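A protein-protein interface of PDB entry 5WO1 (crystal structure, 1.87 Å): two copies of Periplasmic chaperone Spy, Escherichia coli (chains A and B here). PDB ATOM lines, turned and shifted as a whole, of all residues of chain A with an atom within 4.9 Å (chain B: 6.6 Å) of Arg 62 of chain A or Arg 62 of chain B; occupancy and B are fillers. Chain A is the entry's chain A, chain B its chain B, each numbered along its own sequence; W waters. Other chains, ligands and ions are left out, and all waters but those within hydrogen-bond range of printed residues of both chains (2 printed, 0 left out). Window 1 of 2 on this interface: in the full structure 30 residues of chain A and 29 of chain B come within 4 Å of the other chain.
The guanidinium group of Arg 62 of chain B is in salt-bridge range of the side-chain carboxylate of Glu 33 of chain A (3.7 Å).
O of Ile 55 of chain A lies within hydrogen-bond range of NH1 of Arg 62 of chain B.
The guanidinium group (NH2) of Arg 62 of chain A lies within salt-bridge range of the side-chain carboxylate (OE1) of Glu 59 of chain B, 2.8 Å away.
The guanidinium group of Arg 62 of chain B sits close to the guanidinium group of Arg 62 of chain A (2.9 Å).
The guanidinium group (NH2) of Arg 62 of chain A is in hydrogen-bond range of the backbone carbonyl oxygen (O) of Ile 55 of chain A, at 2.9 Å.
The side-chain amino group of Lys 63 of chain B is in salt-bridge range of the side-chain carboxylate of Glu 60 of chain B, at 3.7 Å.
Among the printed residues, pairs that only touch across the chains: Ile 55 of chain A with Lys 63 of chain B (3.9 Å), Ile 55 of chain A with Met 66 of chain B (3.5 Å), Ile 55 of chain A with Leu 67 of chain B (3.6 Å), Lys 63 of chain A with Ile 55 of chain B (3.8 Å), Met 66 of chain A with Ile 55 of chain B (3.6 Å) and Leu 67 of chain A with Ile 55 of chain B (3.6 Å).
Arg 62 of chain A touches just these residues of chain B: Glu 59 (2.8 Å) and Arg 62 (2.9 Å).
Arg 62 of chain B touches just these residues of chain A: Glu 33 (3.7 Å), Ile 55 (3.0 Å) and Arg 62 (2.9 Å).
Printed residues of chain B within 4 Å of Glu 33 of chain A: Arg 62 (3.7 Å).
Printed residues of chain B within 4 Å of Leu 67 of chain A: Ile 55.
Printed residues of chain A within 4 Å of Glu 59 of chain B: Arg 62.
Ala 56 of chain A touches none of the printed residues of chain B.
The nearest printed residue of chain B that does not touch Glu 33 of chain A is Met 66 of chain B (6.9 Å).
Printed residues of chain A that touch a printed residue of chain B: Glu 33, Ile 55, Arg 62, Lys 63, Met 66 and Leu 67.
Of the 13 printed residues of chain B, 6 touch a printed residue of chain A.
Printed residues of chain B that touch a printed residue of chain A: Ile 55, Glu 59, Arg 62, Lys 63, Met 66 and Leu 67.
Hydrophobic or aromatic side chains of chain B that line the printed part of chain A: Ile 55, Met 66 and Leu 67.
Among the printed residues, 10 pairs touch across the chains.
Glu 33 of chain A touches Arg 62 of chain B, but with the chains exchanged Arg 62 of chain A does not touch Glu 33 of chain B (11.8 Å).
Ile 55 of chain A touches Arg 62 of chain B, but with the chains exchanged Arg 62 of chain A does not touch Ile 55 of chain B (5.0 Å).
Ile 55 of chain A touches Met 66 of chain B, and with the chains exchanged Met 66 of chain A touches Ile 55 of chain B.
Arg 62 of chain A touches Glu 59 of chain B, but with the chains exchanged Glu 59 of chain A does not touch Arg 62 of chain B (6.4 Å).
Water W2 lies within hydrogen-bond range of O of Glu 59 of chain A (2.8 Å), OE2 of Glu 59 of chain B (2.8 Å) and N of Lys 63 of chain A (3.4 Å).
Water W1 lies within hydrogen-bond range of the side-chain carboxylate (OE1) of Glu 59 of chain A (2.8 Å) and the side-chain carboxylate (OE1) of Glu 59 of chain B (3.0 Å).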
ATOM      1  N   GLU A  33      -2.060  19.734 -36.051  1.00  0.00           N
ATOM      2  CA  GLU A  33      -3.496  20.028 -35.931  1.00  0.00           C
ATOM      3  C   GLU A  33      -3.855  21.481 -36.304  1.00  0.00           C
ATOM      4  O   GLU A  33      -4.910  21.719 -36.907  1.00  0.00           O
ATOM      5  CB  GLU A  33      -3.990  19.716 -34.506  1.00  0.00           C
ATOM      6  CG  GLU A  33      -5.469  20.176 -34.230  1.00  0.00           C
ATOM      7  CD  GLU A  33      -6.202  19.377 -33.113  1.00  0.00           C
ATOM      8  OE1 GLU A  33      -6.422  18.163 -33.293  1.00  0.00           O
ATOM      9  OE2 GLU A  33      -6.581  19.954 -32.058  1.00  0.00           O
ATOM     10  N   ILE A  55     -11.876  17.896 -36.370  1.00  0.00           N
ATOM     11  CA  ILE A  55     -12.175  18.093 -34.957  1.00  0.00           C
ATOM     12  C   ILE A  55     -12.032  16.766 -34.205  1.00  0.00           C
ATOM     13  O   ILE A  55     -11.564  16.724 -33.056  1.00  0.00           O
ATOM     14  CB  ILE A  55     -13.585  18.702 -34.821  1.00  0.00           C
ATOM     15  CG1 ILE A  55     -13.621  20.155 -35.321  1.00  0.00           C
ATOM     16  CG2 ILE A  55     -14.112  18.582 -33.398  1.00  0.00           C
ATOM     17  CD1 ILE A  55     -15.061  20.667 -35.518  1.00  0.00           C
ATOM     18  N   ALA A  56     -12.424  15.671 -34.846  1.00  0.00           N
ATOM     19  CA  ALA A  56     -12.430  14.369 -34.203  1.00  0.00           C
ATOM     20  C   ALA A  56     -11.070  13.681 -34.190  1.00  0.00           C
ATOM     21  O   ALA A  56     -10.870  12.766 -33.375  1.00  0.00           O
ATOM     22  CB  ALA A  56     -13.438  13.446 -34.884  1.00  0.00           C
ATOM     23  N   MET A  58      -8.038  13.996 -33.096  1.00  0.00           N
ATOM     24  CA  MET A  58      -7.213  13.792 -31.909  1.00  0.00           C
ATOM     25  C   MET A  58      -8.029  13.406 -30.680  1.00  0.00           C
ATOM     26  O   MET A  58      -7.583  13.649 -29.563  1.00  0.00           O
ATOM     27  CB  MET A  58      -6.398  15.046 -31.593  1.00  0.00           C
ATOM     28  CG  MET A  58      -5.578  15.557 -32.763  1.00  0.00           C
ATOM     29  SD  MET A  58      -4.262  14.425 -33.162  1.00  0.00           S
ATOM     30  CE  MET A  58      -3.119  14.923 -31.875  1.00  0.00           C
ATOM     31  N   GLU A  59      -9.216  12.828 -30.857  1.00  0.00           N
ATOM     32  CA  GLU A  59     -10.049  12.452 -29.707  1.00  0.00           C
ATOM     33  C   GLU A  59      -9.299  11.601 -28.674  1.00  0.00           C
ATOM     34  O   GLU A  59      -9.399  11.827 -27.453  1.00  0.00           O
ATOM     35  CB  GLU A  59     -11.260  11.691 -30.235  1.00  0.00           C
ATOM     36  CG  GLU A  59     -12.170  11.138 -29.194  1.00  0.00           C
ATOM     37  CD  GLU A  59     -13.176  10.201 -29.852  1.00  0.00           C
ATOM     38  OE1 GLU A  59     -13.627  10.595 -30.933  1.00  0.00           O
ATOM     39  OE2 GLU A  59     -13.474   9.098 -29.358  1.00  0.00           O
ATOM     40  N   GLU A  60      -8.564  10.582 -29.133  1.00  0.00           N
ATOM     41  CA  GLU A  60      -7.915   9.692 -28.166  1.00  0.00           C
ATOM     42  C   GLU A  60      -6.777  10.389 -27.418  1.00  0.00           C
ATOM     43  O   GLU A  60      -6.571  10.127 -26.231  1.00  0.00           O
ATOM     44  CB  GLU A  60      -7.428   8.416 -28.863  1.00  0.00           C
ATOM     45  CG  GLU A  60      -8.581   7.520 -29.409  1.00  0.00           C
ATOM     46  CD  GLU A  60      -8.199   6.042 -29.600  1.00  0.00           C
ATOM     47  OE1 GLU A  60      -8.218   5.561 -30.754  1.00  0.00           O
ATOM     48  OE2 GLU A  60      -7.872   5.359 -28.594  1.00  0.00           O
ATOM     49  N   GLN A  61      -6.040  11.298 -28.064  1.00  0.00           N
ATOM     50  CA  GLN A  61      -4.985  12.006 -27.337  1.00  0.00           C
ATOM     51  C   GLN A  61      -5.572  13.000 -26.346  1.00  0.00           C
ATOM     52  O   GLN A  61      -5.070  13.144 -25.219  1.00  0.00           O
ATOM     53  CB  GLN A  61      -4.057  12.708 -28.317  1.00  0.00           C
ATOM     54  CG  GLN A  61      -3.373  11.757 -29.300  1.00  0.00           C
ATOM     55  CD  GLN A  61      -4.134  11.568 -30.628  1.00  0.00           C
ATOM     56  OE1 GLN A  61      -5.283  11.096 -30.667  1.00  0.00           O
ATOM     57  NE2 GLN A  61      -3.472  11.934 -31.731  1.00  0.00           N
ATOM     58  N   ARG A  62      -6.639  13.697 -26.747  1.00  0.00           N
ATOM     59  CA  ARG A  62      -7.382  14.553 -25.828  1.00  0.00           C
ATOM     60  C   ARG A  62      -7.881  13.801 -24.603  1.00  0.00           C
ATOM     61  O   ARG A  62      -7.821  14.326 -23.482  1.00  0.00           O
ATOM     62  CB  ARG A  62      -8.570  15.181 -26.535  1.00  0.00           C
ATOM     63  CG  ARG A  62      -8.174  16.250 -27.524  1.00  0.00           C
ATOM     64  CD  ARG A  62      -9.342  17.108 -27.791  1.00  0.00           C
ATOM     65  NE  ARG A  62     -10.397  16.381 -28.501  1.00  0.00           N
ATOM     66  CZ  ARG A  62     -10.411  16.245 -29.822  1.00  0.00           C
ATOM     67  NH1 ARG A  62      -9.449  16.773 -30.553  1.00  0.00           N
ATOM     68  NH2 ARG A  62     -11.379  15.589 -30.423  1.00  0.00           N
ATOM     69  N   LYS A  63      -8.422  12.601 -24.797  1.00  0.00           N
ATOM     70  CA  LYS A  63      -8.907  11.798 -23.667  1.00  0.00           C
ATOM     71  C   LYS A  63      -7.770  11.437 -22.718  1.00  0.00           C
ATOM     72  O   LYS A  63      -7.916  11.508 -21.489  1.00  0.00           O
ATOM     73  CB  LYS A  63      -9.575  10.539 -24.187  1.00  0.00           C
ATOM     74  CG  LYS A  63      -9.974   9.498 -23.126  1.00  0.00           C
ATOM     75  CD  LYS A  63     -10.665   8.268 -23.782  1.00  0.00           C
ATOM     76  CE  LYS A  63     -11.068   7.229 -22.671  1.00  0.00           C
ATOM     77  NZ  LYS A  63     -11.627   6.056 -23.369  1.00  0.00           N
ATOM     78  N   ALA A  64      -6.643  11.000 -23.273  1.00  0.00           N
ATOM     79  CA  ALA A  64      -5.524  10.585 -22.430  1.00  0.00           C
ATOM     80  C   ALA A  64      -5.013  11.772 -21.641  1.00  0.00           C
ATOM     81  O   ALA A  64      -4.755  11.678 -20.443  1.00  0.00           O
ATOM     82  CB  ALA A  64      -4.422   9.986 -23.304  1.00  0.00           C
ATOM     83  N   ASN A  65      -4.937  12.940 -22.294  1.00  0.00           N
ATOM     84  CA  ASN A  65      -4.461  14.147 -21.623  1.00  0.00           C
ATOM     85  C   ASN A  65      -5.430  14.618 -20.555  1.00  0.00           C
ATOM     86  O   ASN A  65      -5.015  14.962 -19.442  1.00  0.00           O
ATOM     87  CB  ASN A  65      -4.222  15.244 -22.650  1.00  0.00           C
ATOM     88  CG  ASN A  65      -3.016  14.948 -23.524  1.00  0.00           C
ATOM     89  OD1 ASN A  65      -2.178  14.091 -23.198  1.00  0.00           O
ATOM     90  ND2 ASN A  65      -2.921  15.651 -24.635  1.00  0.00           N
ATOM     91  N   MET A  66      -6.722  14.671 -20.873  1.00  0.00           N
ATOM     92  CA  MET A  66      -7.706  15.091 -19.882  1.00  0.00           C
ATOM     93  C   MET A  66      -7.684  14.162 -18.681  1.00  0.00           C
ATOM     94  O   MET A  66      -7.553  14.619 -17.539  1.00  0.00           O
ATOM     95  CB  MET A  66      -9.113  15.139 -20.491  1.00  0.00           C
ATOM     96  CG  MET A  66      -9.423  16.404 -21.308  1.00  0.00           C
ATOM     97  SD  MET A  66      -9.050  17.951 -20.440  1.00  0.00           S
ATOM     98  CE  MET A  66      -9.531  17.574 -18.753  1.00  0.00           C
ATOM     99  N   LEU A  67      -7.761  12.851 -18.918  1.00  0.00           N
ATOM    100  CA  LEU A  67      -7.744  11.898 -17.806  1.00  0.00           C
ATOM    101  C   LEU A  67      -6.566  12.142 -16.884  1.00  0.00           C
ATOM    102  O   LEU A  67      -6.697  12.040 -15.659  1.00  0.00           O
ATOM    103  CB  LEU A  67      -7.658  10.475 -18.304  1.00  0.00           C
ATOM    104  CG  LEU A  67      -8.941   9.830 -18.827  1.00  0.00           C
ATOM    105  CD1 LEU A  67      -8.655   8.431 -19.416  1.00  0.00           C
ATOM    106  CD2 LEU A  67      -9.895   9.709 -17.660  1.00  0.00           C
ATOM    107  N   GLU B  33     -21.551  21.180 -17.363  1.00  0.00           N
ATOM    108  CA  GLU B  33     -20.347  20.390 -17.607  1.00  0.00           C
ATOM    109  C   GLU B  33     -19.283  20.658 -16.553  1.00  0.00           C
ATOM    110  O   GLU B  33     -18.694  19.724 -15.990  1.00  0.00           O
ATOM    111  CB  GLU B  33     -19.787  20.729 -18.986  1.00  0.00           C
ATOM    112  CG  GLU B  33     -19.607  19.561 -19.928  1.00  0.00           C
ATOM    113  CD  GLU B  33     -20.104  19.882 -21.329  1.00  0.00           C
ATOM    114  OE1 GLU B  33     -19.392  20.605 -22.056  1.00  0.00           O
ATOM    115  OE2 GLU B  33     -21.216  19.442 -21.689  1.00  0.00           O
ATOM    116  N   ILE B  55     -15.422  13.354 -20.110  1.00  0.00           N
ATOM    117  CA  ILE B  55     -14.645  13.725 -21.308  1.00  0.00           C
ATOM    118  C   ILE B  55     -15.464  13.530 -22.575  1.00  0.00           C
ATOM    119  O   ILE B  55     -15.513  14.399 -23.461  1.00  0.00           O
ATOM    120  CB  ILE B  55     -13.337  12.915 -21.374  1.00  0.00           C
ATOM    121  CG1 ILE B  55     -12.432  13.359 -20.244  1.00  0.00           C
ATOM    122  CG2 ILE B  55     -12.656  13.064 -22.799  1.00  0.00           C
ATOM    123  CD1 ILE B  55     -11.279  12.364 -19.931  1.00  0.00           C
ATOM    124  N   LYS B  57     -18.696  13.507 -22.957  1.00  0.00           N
ATOM    125  CA  LYS B  57     -19.740  14.518 -23.034  1.00  0.00           C
ATOM    126  C   LYS B  57     -19.147  15.848 -23.477  1.00  0.00           C
ATOM    127  O   LYS B  57     -19.716  16.527 -24.344  1.00  0.00           O
ATOM    128  CB  LYS B  57     -20.462  14.654 -21.684  1.00  0.00           C
ATOM    129  CG  LYS B  57     -21.974  14.783 -21.719  1.00  0.00           C
ATOM    130  CD  LYS B  57     -22.409  16.082 -22.344  1.00  0.00           C
ATOM    131  CE  LYS B  57     -23.859  16.025 -22.862  1.00  0.00           C
ATOM    132  NZ  LYS B  57     -24.843  15.791 -21.769  1.00  0.00           N
ATOM    133  N   MET B  58     -17.955  16.198 -22.966  1.00  0.00           N
ATOM    134  CA  MET B  58     -17.304  17.447 -23.383  1.00  0.00           C
ATOM    135  C   MET B  58     -16.960  17.483 -24.872  1.00  0.00           C
ATOM    136  O   MET B  58     -16.906  18.573 -25.450  1.00  0.00           O
ATOM    137  CB  MET B  58     -16.039  17.668 -22.568  1.00  0.00           C
ATOM    138  CG  MET B  58     -16.311  18.080 -21.115  1.00  0.00           C
ATOM    139  SD  MET B  58     -14.848  17.853 -20.072  1.00  0.00           S
ATOM    140  CE  MET B  58     -15.529  18.379 -18.482  1.00  0.00           C
ATOM    141  N   GLU B  59     -16.737  16.332 -25.516  1.00  0.00           N
ATOM    142  CA  GLU B  59     -16.490  16.310 -26.967  1.00  0.00           C
ATOM    143  C   GLU B  59     -17.656  16.881 -27.781  1.00  0.00           C
ATOM    144  O   GLU B  59     -17.429  17.432 -28.870  1.00  0.00           O
ATOM    145  CB  GLU B  59     -16.184  14.884 -27.418  1.00  0.00           C
ATOM    146  CG  GLU B  59     -14.816  14.347 -26.937  1.00  0.00           C
ATOM    147  CD  GLU B  59     -13.620  14.940 -27.691  1.00  0.00           C
ATOM    148  OE1 GLU B  59     -13.711  15.189 -28.898  1.00  0.00           O
ATOM    149  OE2 GLU B  59     -12.560  15.152 -27.093  1.00  0.00           O
ATOM    150  N   GLU B  60     -18.907  16.744 -27.309  1.00  0.00           N
ATOM    151  CA  GLU B  60     -20.004  17.277 -28.111  1.00  0.00           C
ATOM    152  C   GLU B  60     -20.028  18.802 -28.063  1.00  0.00           C
ATOM    153  O   GLU B  60     -20.286  19.431 -29.095  1.00  0.00           O
ATOM    154  CB  GLU B  60     -21.352  16.669 -27.686  1.00  0.00           C
ATOM    155  CG  GLU B  60     -22.633  17.230 -28.392  1.00  0.00           C
ATOM    156  CD  GLU B  60     -22.918  16.755 -29.859  1.00  0.00           C
ATOM    157  OE1 GLU B  60     -22.100  16.104 -30.521  1.00  0.00           O
ATOM    158  OE2 GLU B  60     -24.016  17.061 -30.349  1.00  0.00           O
ATOM    159  N   GLN B  61     -19.744  19.419 -26.909  1.00  0.00           N
ATOM    160  CA  GLN B  61     -19.701  20.875 -26.861  1.00  0.00           C
ATOM    161  C   GLN B  61     -18.508  21.394 -27.645  1.00  0.00           C
ATOM    162  O   GLN B  61     -18.616  22.395 -28.368  1.00  0.00           O
ATOM    163  CB  GLN B  61     -19.651  21.380 -25.407  1.00  0.00           C
ATOM    164  CG  GLN B  61     -20.164  22.798 -25.255  1.00  0.00           C
ATOM    165  CD  GLN B  61     -21.600  22.927 -25.732  1.00  0.00           C
ATOM    166  OE1 GLN B  61     -21.918  23.754 -26.598  1.00  0.00           O
ATOM    167  NE2 GLN B  61     -22.475  22.079 -25.190  1.00  0.00           N
ATOM    168  N   ARG B  62     -17.361  20.738 -27.496  1.00  0.00           N
ATOM    169  CA  ARG B  62     -16.185  21.129 -28.256  1.00  0.00           C
ATOM    170  C   ARG B  62     -16.424  21.052 -29.758  1.00  0.00           C
ATOM    171  O   ARG B  62     -15.958  21.914 -30.517  1.00  0.00           O
ATOM    172  CB  ARG B  62     -15.014  20.240 -27.872  1.00  0.00           C
ATOM    173  CG  ARG B  62     -13.756  20.500 -28.682  1.00  0.00           C
ATOM    174  CD  ARG B  62     -12.561  19.654 -28.204  1.00  0.00           C
ATOM    175  NE  ARG B  62     -11.369  19.878 -29.028  1.00  0.00           N
ATOM    176  CZ  ARG B  62     -11.196  19.347 -30.237  1.00  0.00           C
ATOM    177  NH1 ARG B  62     -12.131  18.576 -30.761  1.00  0.00           N
ATOM    178  NH2 ARG B  62     -10.093  19.597 -30.929  1.00  0.00           N
ATOM    179  N   LYS B  63     -17.125  20.019 -30.223  1.00  0.00           N
ATOM    180  CA  LYS B  63     -17.397  19.922 -31.642  1.00  0.00           C
ATOM    181  C   LYS B  63     -18.210  21.108 -32.092  1.00  0.00           C
ATOM    182  O   LYS B  63     -17.902  21.759 -33.101  1.00  0.00           O
ATOM    183  CB  LYS B  63     -18.144  18.629 -31.941  1.00  0.00           C
ATOM    184  CG  LYS B  63     -18.601  18.420 -33.430  1.00  0.00           C
ATOM    185  CD  LYS B  63     -19.761  17.399 -33.403  1.00  0.00           C
ATOM    186  CE  LYS B  63     -20.291  16.879 -34.669  1.00  0.00           C
ATOM    187  NZ  LYS B  63     -21.547  16.174 -34.223  1.00  0.00           N
ATOM    188  N   ALA B  64     -19.279  21.399 -31.359  1.00  0.00           N
ATOM    189  CA  ALA B  64     -20.103  22.552 -31.705  1.00  0.00           C
ATOM    190  C   ALA B  64     -19.282  23.837 -31.730  1.00  0.00           C
ATOM    191  O   ALA B  64     -19.399  24.648 -32.659  1.00  0.00           O
ATOM    192  CB  ALA B  64     -21.252  22.662 -30.704  1.00  0.00           C
ATOM    193  N   ASN B  65     -18.456  24.041 -30.701  1.00  0.00           N
ATOM    194  CA  ASN B  65     -17.704  25.279 -30.567  1.00  0.00           C
ATOM    195  C   ASN B  65     -16.643  25.397 -31.649  1.00  0.00           C
ATOM    196  O   ASN B  65     -16.427  26.481 -32.196  1.00  0.00           O
ATOM    197  CB  ASN B  65     -17.051  25.352 -29.193  1.00  0.00           C
ATOM    198  CG  ASN B  65     -18.045  25.591 -28.085  1.00  0.00           C
ATOM    199  OD1 ASN B  65     -19.117  26.164 -28.299  1.00  0.00           O
ATOM    200  ND2 ASN B  65     -17.678  25.175 -26.876  1.00  0.00           N
ATOM    201  N   MET B  66     -15.952  24.296 -31.949  1.00  0.00           N
ATOM    202  CA  MET B  66     -14.970  24.332 -33.023  1.00  0.00           C
ATOM    203  C   MET B  66     -15.621  24.587 -34.372  1.00  0.00           C
ATOM    204  O   MET B  66     -15.107  25.385 -35.153  1.00  0.00           O
ATOM    205  CB  MET B  66     -14.161  23.046 -33.060  1.00  0.00           C
ATOM    206  CG  MET B  66     -13.204  22.929 -31.854  1.00  0.00           C
ATOM    207  SD  MET B  66     -12.108  24.347 -31.651  1.00  0.00           S
ATOM    208  CE  MET B  66     -11.487  24.569 -33.307  1.00  0.00           C
ATOM    209  N   LEU B  67     -16.728  23.897 -34.684  1.00  0.00           N
ATOM    210  CA  LEU B  67     -17.394  24.123 -35.970  1.00  0.00           C
ATOM    211  C   LEU B  67     -17.803  25.574 -36.123  1.00  0.00           C
ATOM    212  O   LEU B  67     -17.675  26.148 -37.216  1.00  0.00           O
ATOM    213  CB  LEU B  67     -18.627  23.225 -36.126  1.00  0.00           C
ATOM    214  CG  LEU B  67     -18.385  21.755 -36.412  1.00  0.00           C
ATOM    215  CD1 LEU B  67     -19.689  20.912 -36.301  1.00  0.00           C
ATOM    216  CD2 LEU B  67     -17.848  21.694 -37.827  1.00  0.00           C
HETATM  217  O   HOH W   1     -14.658  13.222 -30.932  1.00  0.00           O
HETATM  218  O   HOH W   2     -11.589  12.741 -26.036  1.00  0.00           O
